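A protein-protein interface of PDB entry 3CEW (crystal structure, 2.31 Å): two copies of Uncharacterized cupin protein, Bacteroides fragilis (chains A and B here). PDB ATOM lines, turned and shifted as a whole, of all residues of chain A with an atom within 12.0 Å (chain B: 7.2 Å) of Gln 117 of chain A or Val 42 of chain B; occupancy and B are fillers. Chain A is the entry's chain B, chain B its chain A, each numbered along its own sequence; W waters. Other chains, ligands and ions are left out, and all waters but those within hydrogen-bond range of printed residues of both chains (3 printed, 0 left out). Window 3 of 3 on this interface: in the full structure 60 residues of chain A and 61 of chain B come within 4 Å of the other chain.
Among the printed residues, pairs that only touch across the chains: Val 115 of chain A with His 43 of chain B (3.1 Å), Gly 114 of chain A with Ser 44 of chain B (3.4 Å), Val 116 of chain A with Val 42 of chain B (3.5 Å), Gln 117 of chain A with Lys 83 of chain B (3.6 Å), Asn 3 of chain A with Gly 82 of chain B (3.7 Å), Gly 114 of chain A with His 45 of chain B (3.7 Å) and Asn 3 of chain A with Asp 81 of chain B (3.9 Å).
Of the printed residues of chain B, Gly 114 of chain A touches Ser 44 and His 45.
Of the printed residues of chain B, Val 116 of chain A touches Val 42 (3.5 Å).
Gln 117 of chain A touches just these residues of chain B: Val 42, Ser 44 and Lys 83.
No residue of chain A comes within 4 Å of Phe 41 of chain B.
Printed residues of chain A within 4 Å of His 45 of chain B: Asp 113 and Gly 114.
Printed residues of chain A within 4 Å of Gly 82 of chain B: Asn 3 (3.7 Å).
Of the printed residues of chain A, Lys 83 of chain B touches Gln 117.
Ile 86 of chain B touches none of the printed residues of chain A.
The nearest residue of chain A that does not touch Val 42 of chain B is Val 115 of chain A (4.1 Å).
The nearest printed residue of chain A that does not touch Gly 82 of chain B is Gln 117 of chain A (6.4 Å).
O of His 43 of chain B sits at hydrogen-bond distance from N of Arg 84 of chain B (2.9 Å).
The backbone NH (N) of Asp 64 of chain B lies within hydrogen-bond range of the backbone carbonyl oxygen (O) of Lys 83 of chain B (2.8 Å).
The backbone carbonyl oxygen (O) of Gly 82 of chain B sits at hydrogen-bond distance from the guanidinium group (NH1) of Arg 84 of chain B (2.7 Å).
OE1 of Gln 117 of chain A lies close to O of Val 115 of chain A (3.4 Å).
Hydrophobic or aromatic side chains of chain A within 4 Å of the printed part of chain B: Val 115 and Val 116.
No position is printed for both chains.
N of Gln 117 of chain A is in hydrogen-bond range of O of Val 42 of chain B (2.9 Å).
The backbone carbonyl oxygen (O) of Ser 44 of chain B sits at hydrogen-bond distance from the backbone NH (N) of Val 115 of chain A (2.7 Å).
OE1 of Gln 117 of chain A sits at hydrogen-bond distance from OG of Ser 44 of chain B (3.3 Å).
ND1 of His 45 of chain B sits at hydrogen-bond distance from OD1 of Asp 113 of chain A (2.7 Å).
The side-chain carboxylate (OD2) of Asp 64 of chain B sits close to the side-chain amide oxygen (OD1) of Asn 3 of chain A (2.9 Å).
Water W1 lies within hydrogen-bond range of ND2 of Asn 3 of chain A and OD2 of Asp 81 of chain B.
Water W2 bridges O of Gln 117 of chain A (2.7 Å) and N of Val 42 of chain B (3.0 Å).
Water W3 bridges OD2 of Asp 64 of chain B (3.0 Å) and N of Asn 3 of chain A (3.0 Å).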
ATOM      1  N   ASN A   3      30.009  11.858  -8.236  1.00  0.00           N
ATOM      2  CA  ASN A   3      28.973  11.104  -7.549  1.00  0.00           C
ATOM      3  C   ASN A   3      28.899   9.673  -8.065  1.00  0.00           C
ATOM      4  O   ASN A   3      27.898   8.991  -7.867  1.00  0.00           O
ATOM      5  CB  ASN A   3      27.616  11.783  -7.731  1.00  0.00           C
ATOM      6  CG  ASN A   3      27.405  12.939  -6.769  1.00  0.00           C
ATOM      7  OD1 ASN A   3      26.809  13.950  -7.130  1.00  0.00           O
ATOM      8  ND2 ASN A   3      27.872  12.787  -5.533  1.00  0.00           N
ATOM      9  N   THR A 110      12.869   2.939  -4.599  1.00  0.00           N
ATOM     10  CA  THR A 110      12.129   3.278  -5.812  1.00  0.00           C
ATOM     11  C   THR A 110      11.158   4.418  -5.516  1.00  0.00           C
ATOM     12  O   THR A 110      11.581   5.559  -5.307  1.00  0.00           O
ATOM     13  CB  THR A 110      11.359   2.040  -6.352  1.00  0.00           C
ATOM     14  OG1 THR A 110      12.243   0.911  -6.400  1.00  0.00           O
ATOM     15  CG2 THR A 110      10.834   2.302  -7.762  1.00  0.00           C
ATOM     16  N   MET A 111       9.867   4.111  -5.479  1.00  0.00           N
ATOM     17  CA  MET A 111       8.850   5.122  -5.189  1.00  0.00           C
ATOM     18  C   MET A 111       9.099   5.864  -3.880  1.00  0.00           C
ATOM     19  O   MET A 111       8.862   7.063  -3.784  1.00  0.00           O
ATOM     20  CB  MET A 111       7.467   4.475  -5.127  1.00  0.00           C
ATOM     21  CG  MET A 111       6.757   4.370  -6.456  1.00  0.00           C
ATOM     22  SD  MET A 111       5.965   6.053  -6.954  1.00  0.00           S
ATOM     23  CE  MET A 111       4.305   5.888  -5.980  1.00  0.00           C
ATOM     24  N   ASP A 113      12.059   6.369  -2.391  1.00  0.00           N
ATOM     25  CA  ASP A 113      13.442   6.834  -2.249  1.00  0.00           C
ATOM     26  C   ASP A 113      13.983   7.592  -3.467  1.00  0.00           C
ATOM     27  O   ASP A 113      14.889   8.415  -3.341  1.00  0.00           O
ATOM     28  CB  ASP A 113      14.390   5.682  -1.912  1.00  0.00           C
ATOM     29  CG  ASP A 113      15.770   6.172  -1.489  1.00  0.00           C
ATOM     30  OD1 ASP A 113      16.689   6.252  -2.332  1.00  0.00           O
ATOM     31  OD2 ASP A 113      15.930   6.499  -0.298  1.00  0.00           O
ATOM     32  N   GLY A 114      13.432   7.318  -4.645  1.00  0.00           N
ATOM     33  CA  GLY A 114      13.882   8.015  -5.837  1.00  0.00           C
ATOM     34  C   GLY A 114      13.320   9.427  -5.903  1.00  0.00           C
ATOM     35  O   GLY A 114      12.215   9.694  -5.423  1.00  0.00           O
ATOM     36  N   VAL A 115      14.083  10.337  -6.496  1.00  0.00           N
ATOM     37  CA  VAL A 115      13.652  11.721  -6.639  1.00  0.00           C
ATOM     38  C   VAL A 115      13.809  12.151  -8.091  1.00  0.00           C
ATOM     39  O   VAL A 115      14.920  12.178  -8.622  1.00  0.00           O
ATOM     40  CB  VAL A 115      14.478  12.667  -5.732  1.00  0.00           C
ATOM     41  CG1 VAL A 115      14.040  14.121  -5.946  1.00  0.00           C
ATOM     42  CG2 VAL A 115      14.302  12.265  -4.271  1.00  0.00           C
ATOM     43  N   VAL A 116      12.687  12.474  -8.725  1.00  0.00           N
ATOM     44  CA  VAL A 116      12.686  12.900 -10.117  1.00  0.00           C
ATOM     45  C   VAL A 116      13.153  14.340 -10.228  1.00  0.00           C
ATOM     46  O   VAL A 116      12.783  15.191  -9.416  1.00  0.00           O
ATOM     47  CB  VAL A 116      11.279  12.794 -10.736  1.00  0.00           C
ATOM     48  CG1 VAL A 116      11.304  13.270 -12.190  1.00  0.00           C
ATOM     49  CG2 VAL A 116      10.792  11.357 -10.661  1.00  0.00           C
ATOM     50  N   GLN A 117      13.954  14.611 -11.247  1.00  0.00           N
ATOM     51  CA  GLN A 117      14.469  15.953 -11.461  1.00  0.00           C
ATOM     52  C   GLN A 117      13.714  16.642 -12.594  1.00  0.00           C
ATOM     53  O   GLN A 117      13.653  16.124 -13.705  1.00  0.00           O
ATOM     54  CB  GLN A 117      15.962  15.881 -11.785  1.00  0.00           C
ATOM     55  CG  GLN A 117      16.848  16.627 -10.803  1.00  0.00           C
ATOM     56  CD  GLN A 117      16.650  16.184  -9.356  1.00  0.00           C
ATOM     57  OE1 GLN A 117      16.734  14.993  -9.032  1.00  0.00           O
ATOM     58  NE2 GLN A 117      16.398  17.149  -8.478  1.00  0.00           N
ATOM     59  N   LEU A 118      13.129  17.802 -12.313  1.00  0.00           N
ATOM     60  CA  LEU A 118      12.397  18.535 -13.345  1.00  0.00           C
ATOM     61  C   LEU A 118      13.331  19.276 -14.299  1.00  0.00           C
ATOM     62  O   LEU A 118      14.563  19.198 -14.099  1.00  0.00           O
ATOM     63  CB  LEU A 118      11.423  19.532 -12.714  1.00  0.00           C
ATOM     64  CG  LEU A 118      10.222  18.904 -12.006  1.00  0.00           C
ATOM     65  CD1 LEU A 118       9.300  20.001 -11.483  1.00  0.00           C
ATOM     66  CD2 LEU A 118       9.477  18.000 -12.978  1.00  0.00           C
ATOM     67  N   VAL B  39      15.650   5.830 -20.513  1.00  0.00           N
ATOM     68  CA  VAL B  39      14.751   6.228 -19.439  1.00  0.00           C
ATOM     69  C   VAL B  39      14.349   7.671 -19.731  1.00  0.00           C
ATOM     70  O   VAL B  39      15.202   8.542 -19.893  1.00  0.00           O
ATOM     71  CB  VAL B  39      15.443   6.130 -18.074  1.00  0.00           C
ATOM     72  CG1 VAL B  39      14.488   6.556 -16.963  1.00  0.00           C
ATOM     73  CG2 VAL B  39      15.904   4.703 -17.844  1.00  0.00           C
ATOM     74  N   PRO B  40      13.039   7.936 -19.820  1.00  0.00           N
ATOM     75  CA  PRO B  40      12.493   9.267 -20.108  1.00  0.00           C
ATOM     76  C   PRO B  40      12.631  10.336 -19.031  1.00  0.00           C
ATOM     77  O   PRO B  40      12.100  11.436 -19.178  1.00  0.00           O
ATOM     78  CB  PRO B  40      11.030   8.974 -20.442  1.00  0.00           C
ATOM     79  CG  PRO B  40      10.715   7.830 -19.533  1.00  0.00           C
ATOM     80  CD  PRO B  40      11.954   6.952 -19.651  1.00  0.00           C
ATOM     81  N   PHE B  41      13.341  10.031 -17.952  1.00  0.00           N
ATOM     82  CA  PHE B  41      13.504  11.020 -16.900  1.00  0.00           C
ATOM     83  C   PHE B  41      14.837  10.881 -16.169  1.00  0.00           C
ATOM     84  O   PHE B  41      15.542   9.881 -16.315  1.00  0.00           O
ATOM     85  CB  PHE B  41      12.340  10.920 -15.905  1.00  0.00           C
ATOM     86  CG  PHE B  41      12.273   9.608 -15.174  1.00  0.00           C
ATOM     87  CD1 PHE B  41      12.992   9.420 -14.006  1.00  0.00           C
ATOM     88  CD2 PHE B  41      11.507   8.551 -15.673  1.00  0.00           C
ATOM     89  CE1 PHE B  41      12.957   8.200 -13.335  1.00  0.00           C
ATOM     90  CE2 PHE B  41      11.460   7.323 -15.014  1.00  0.00           C
ATOM     91  CZ  PHE B  41      12.190   7.144 -13.837  1.00  0.00           C
ATOM     92  N   VAL B  42      15.173  11.904 -15.395  1.00  0.00           N
ATOM     93  CA  VAL B  42      16.404  11.927 -14.618  1.00  0.00           C
ATOM     94  C   VAL B  42      16.034  11.808 -13.143  1.00  0.00           C
ATOM     95  O   VAL B  42      15.025  12.360 -12.711  1.00  0.00           O
ATOM     96  CB  VAL B  42      17.161  13.259 -14.813  1.00  0.00           C
ATOM     97  CG1 VAL B  42      18.392  13.302 -13.907  1.00  0.00           C
ATOM     98  CG2 VAL B  42      17.554  13.421 -16.267  1.00  0.00           C
ATOM     99  N   HIS B  43      16.835  11.094 -12.362  1.00  0.00           N
ATOM    100  CA  HIS B  43      16.519  10.981 -10.946  1.00  0.00           C
ATOM    101  C   HIS B  43      17.728  10.745 -10.069  1.00  0.00           C
ATOM    102  O   HIS B  43      18.782  10.329 -10.523  1.00  0.00           O
ATOM    103  CB  HIS B  43      15.496   9.859 -10.695  1.00  0.00           C
ATOM    104  CG  HIS B  43      16.082   8.484 -10.744  1.00  0.00           C
ATOM    105  ND1 HIS B  43      16.509   7.898 -11.916  1.00  0.00           N
ATOM    106  CD2 HIS B  43      16.343   7.590  -9.760  1.00  0.00           C
ATOM    107  CE1 HIS B  43      17.010   6.704 -11.654  1.00  0.00           C
ATOM    108  NE2 HIS B  43      16.922   6.491 -10.352  1.00  0.00           N
ATOM    109  N   SER B  44      17.534  11.028  -8.793  1.00  0.00           N
ATOM    110  CA  SER B  44      18.543  10.831  -7.779  1.00  0.00           C
ATOM    111  C   SER B  44      17.849  10.068  -6.661  1.00  0.00           C
ATOM    112  O   SER B  44      16.677   9.689  -6.793  1.00  0.00           O
ATOM    113  CB  SER B  44      19.082  12.176  -7.275  1.00  0.00           C
ATOM    114  OG  SER B  44      18.053  12.971  -6.739  1.00  0.00           O
ATOM    115  N   HIS B  45      18.561   9.848  -5.562  1.00  0.00           N
ATOM    116  CA  HIS B  45      18.003   9.119  -4.427  1.00  0.00           C
ATOM    117  C   HIS B  45      18.205   9.851  -3.114  1.00  0.00           C
ATOM    118  O   HIS B  45      19.144  10.619  -2.968  1.00  0.00           O
ATOM    119  CB  HIS B  45      18.633   7.731  -4.350  1.00  0.00           C
ATOM    120  CG  HIS B  45      18.049   6.762  -5.323  1.00  0.00           C
ATOM    121  ND1 HIS B  45      16.930   6.010  -5.036  1.00  0.00           N
ATOM    122  CD2 HIS B  45      18.369   6.488  -6.608  1.00  0.00           C
ATOM    123  CE1 HIS B  45      16.583   5.317  -6.107  1.00  0.00           C
ATOM    124  NE2 HIS B  45      17.440   5.592  -7.074  1.00  0.00           N
ATOM    125  N   THR B  62      24.023   9.253 -18.271  1.00  0.00           N
ATOM    126  CA  THR B  62      24.408  10.615 -17.965  1.00  0.00           C
ATOM    127  C   THR B  62      24.293  10.814 -16.467  1.00  0.00           C
ATOM    128  O   THR B  62      23.223  10.614 -15.882  1.00  0.00           O
ATOM    129  CB  THR B  62      23.513  11.646 -18.696  1.00  0.00           C
ATOM    130  OG1 THR B  62      23.623  11.460 -20.114  1.00  0.00           O
ATOM    131  CG2 THR B  62      23.941  13.073 -18.338  1.00  0.00           C
ATOM    132  N   ASP B  64      24.965  13.644 -13.598  1.00  0.00           N
ATOM    133  CA  ASP B  64      25.252  15.039 -13.299  1.00  0.00           C
ATOM    134  C   ASP B  64      25.814  15.797 -14.517  1.00  0.00           C
ATOM    135  O   ASP B  64      26.857  16.448 -14.432  1.00  0.00           O
ATOM    136  CB  ASP B  64      26.231  15.120 -12.115  1.00  0.00           C
ATOM    137  CG  ASP B  64      25.620  14.618 -10.805  1.00  0.00           C
ATOM    138  OD1 ASP B  64      24.431  14.908 -10.542  1.00  0.00           O
ATOM    139  OD2 ASP B  64      26.331  13.946 -10.022  1.00  0.00           O
ATOM    140  N   ASP B  81      23.094  11.491  -4.270  1.00  0.00           N
ATOM    141  CA  ASP B  81      22.965  12.799  -4.914  1.00  0.00           C
ATOM    142  C   ASP B  81      23.149  12.804  -6.432  1.00  0.00           C
ATOM    143  O   ASP B  81      22.734  13.738  -7.106  1.00  0.00           O
ATOM    144  CB  ASP B  81      23.952  13.801  -4.296  1.00  0.00           C
ATOM    145  CG  ASP B  81      23.647  14.100  -2.841  1.00  0.00           C
ATOM    146  OD1 ASP B  81      22.450  14.219  -2.498  1.00  0.00           O
ATOM    147  OD2 ASP B  81      24.605  14.236  -2.045  1.00  0.00           O
ATOM    148  N   GLY B  82      23.777  11.771  -6.974  1.00  0.00           N
ATOM    149  CA  GLY B  82      23.968  11.728  -8.412  1.00  0.00           C
ATOM    150  C   GLY B  82      22.668  11.732  -9.201  1.00  0.00           C
ATOM    151  O   GLY B  82      21.749  10.959  -8.911  1.00  0.00           O
ATOM    152  N   LYS B  83      22.580  12.623 -10.190  1.00  0.00           N
ATOM    153  CA  LYS B  83      21.411  12.710 -11.066  1.00  0.00           C
ATOM    154  C   LYS B  83      21.753  11.822 -12.255  1.00  0.00           C
ATOM    155  O   LYS B  83      22.685  12.108 -13.008  1.00  0.00           O
ATOM    156  CB  LYS B  83      21.184  14.151 -11.518  1.00  0.00           C
ATOM    157  CG  LYS B  83      20.799  15.088 -10.387  1.00  0.00           C
ATOM    158  CD  LYS B  83      20.581  16.508 -10.893  1.00  0.00           C
ATOM    159  CE  LYS B  83      20.231  17.460  -9.754  1.00  0.00           C
ATOM    160  NZ  LYS B  83      21.316  17.524  -8.728  1.00  0.00           N
ATOM    161  N   ARG B  84      20.987  10.751 -12.430  1.00  0.00           N
ATOM    162  CA  ARG B  84      21.273   9.787 -13.482  1.00  0.00           C
ATOM    163  C   ARG B  84      20.161   9.559 -14.487  1.00  0.00           C
ATOM    164  O   ARG B  84      18.989   9.791 -14.202  1.00  0.00           O
ATOM    165  CB  ARG B  84      21.619   8.447 -12.839  1.00  0.00           C
ATOM    166  CG  ARG B  84      20.387   7.751 -12.264  1.00  0.00           C
ATOM    167  CD  ARG B  84      20.662   7.041 -10.952  1.00  0.00           C
ATOM    168  NE  ARG B  84      20.933   7.981  -9.867  1.00  0.00           N
ATOM    169  CZ  ARG B  84      21.226   7.612  -8.624  1.00  0.00           C
ATOM    170  NH1 ARG B  84      21.464   8.532  -7.695  1.00  0.00           N
ATOM    171  NH2 ARG B  84      21.290   6.323  -8.309  1.00  0.00           N
ATOM    172  N   GLN B  85      20.555   9.067 -15.659  1.00  0.00           N
ATOM    173  CA  GLN B  85      19.628   8.764 -16.743  1.00  0.00           C
ATOM    174  C   GLN B  85      20.373   7.901 -17.758  1.00  0.00           C
ATOM    175  O   GLN B  85      21.292   8.368 -18.426  1.00  0.00           O
ATOM    176  CB  GLN B  85      19.133  10.051 -17.410  1.00  0.00           C
ATOM    177  CG  GLN B  85      18.259   9.805 -18.639  1.00  0.00           C
ATOM    178  CD  GLN B  85      17.617  11.072 -19.178  1.00  0.00           C
ATOM    179  OE1 GLN B  85      18.295  12.074 -19.395  1.00  0.00           O
ATOM    180  NE2 GLN B  85      16.302  11.031 -19.394  1.00  0.00           N
ATOM    181  N   ILE B  86      19.981   6.637 -17.853  1.00  0.00           N
ATOM    182  CA  ILE B  86      20.615   5.705 -18.771  1.00  0.00           C
ATOM    183  C   ILE B  86      19.829   5.581 -20.080  1.00  0.00           C
ATOM    184  O   ILE B  86      18.622   5.827 -20.123  1.00  0.00           O
ATOM    185  CB  ILE B  86      20.756   4.299 -18.114  1.00  0.00           C
ATOM    186  CG1 ILE B  86      21.480   3.340 -19.067  1.00  0.00           C
ATOM    187  CG2 ILE B  86      19.372   3.736 -17.783  1.00  0.00           C
ATOM    188  CD1 ILE B  86      21.752   1.979 -18.464  1.00  0.00           C
HETATM  189  O   HOH W   1      27.419  13.310  -2.902  1.00  0.00           O
HETATM  190  O   HOH W   2      13.465  14.352 -15.774  1.00  0.00           O
HETATM  191  O   HOH W   3      29.250  13.641 -10.578  1.00  0.00           O
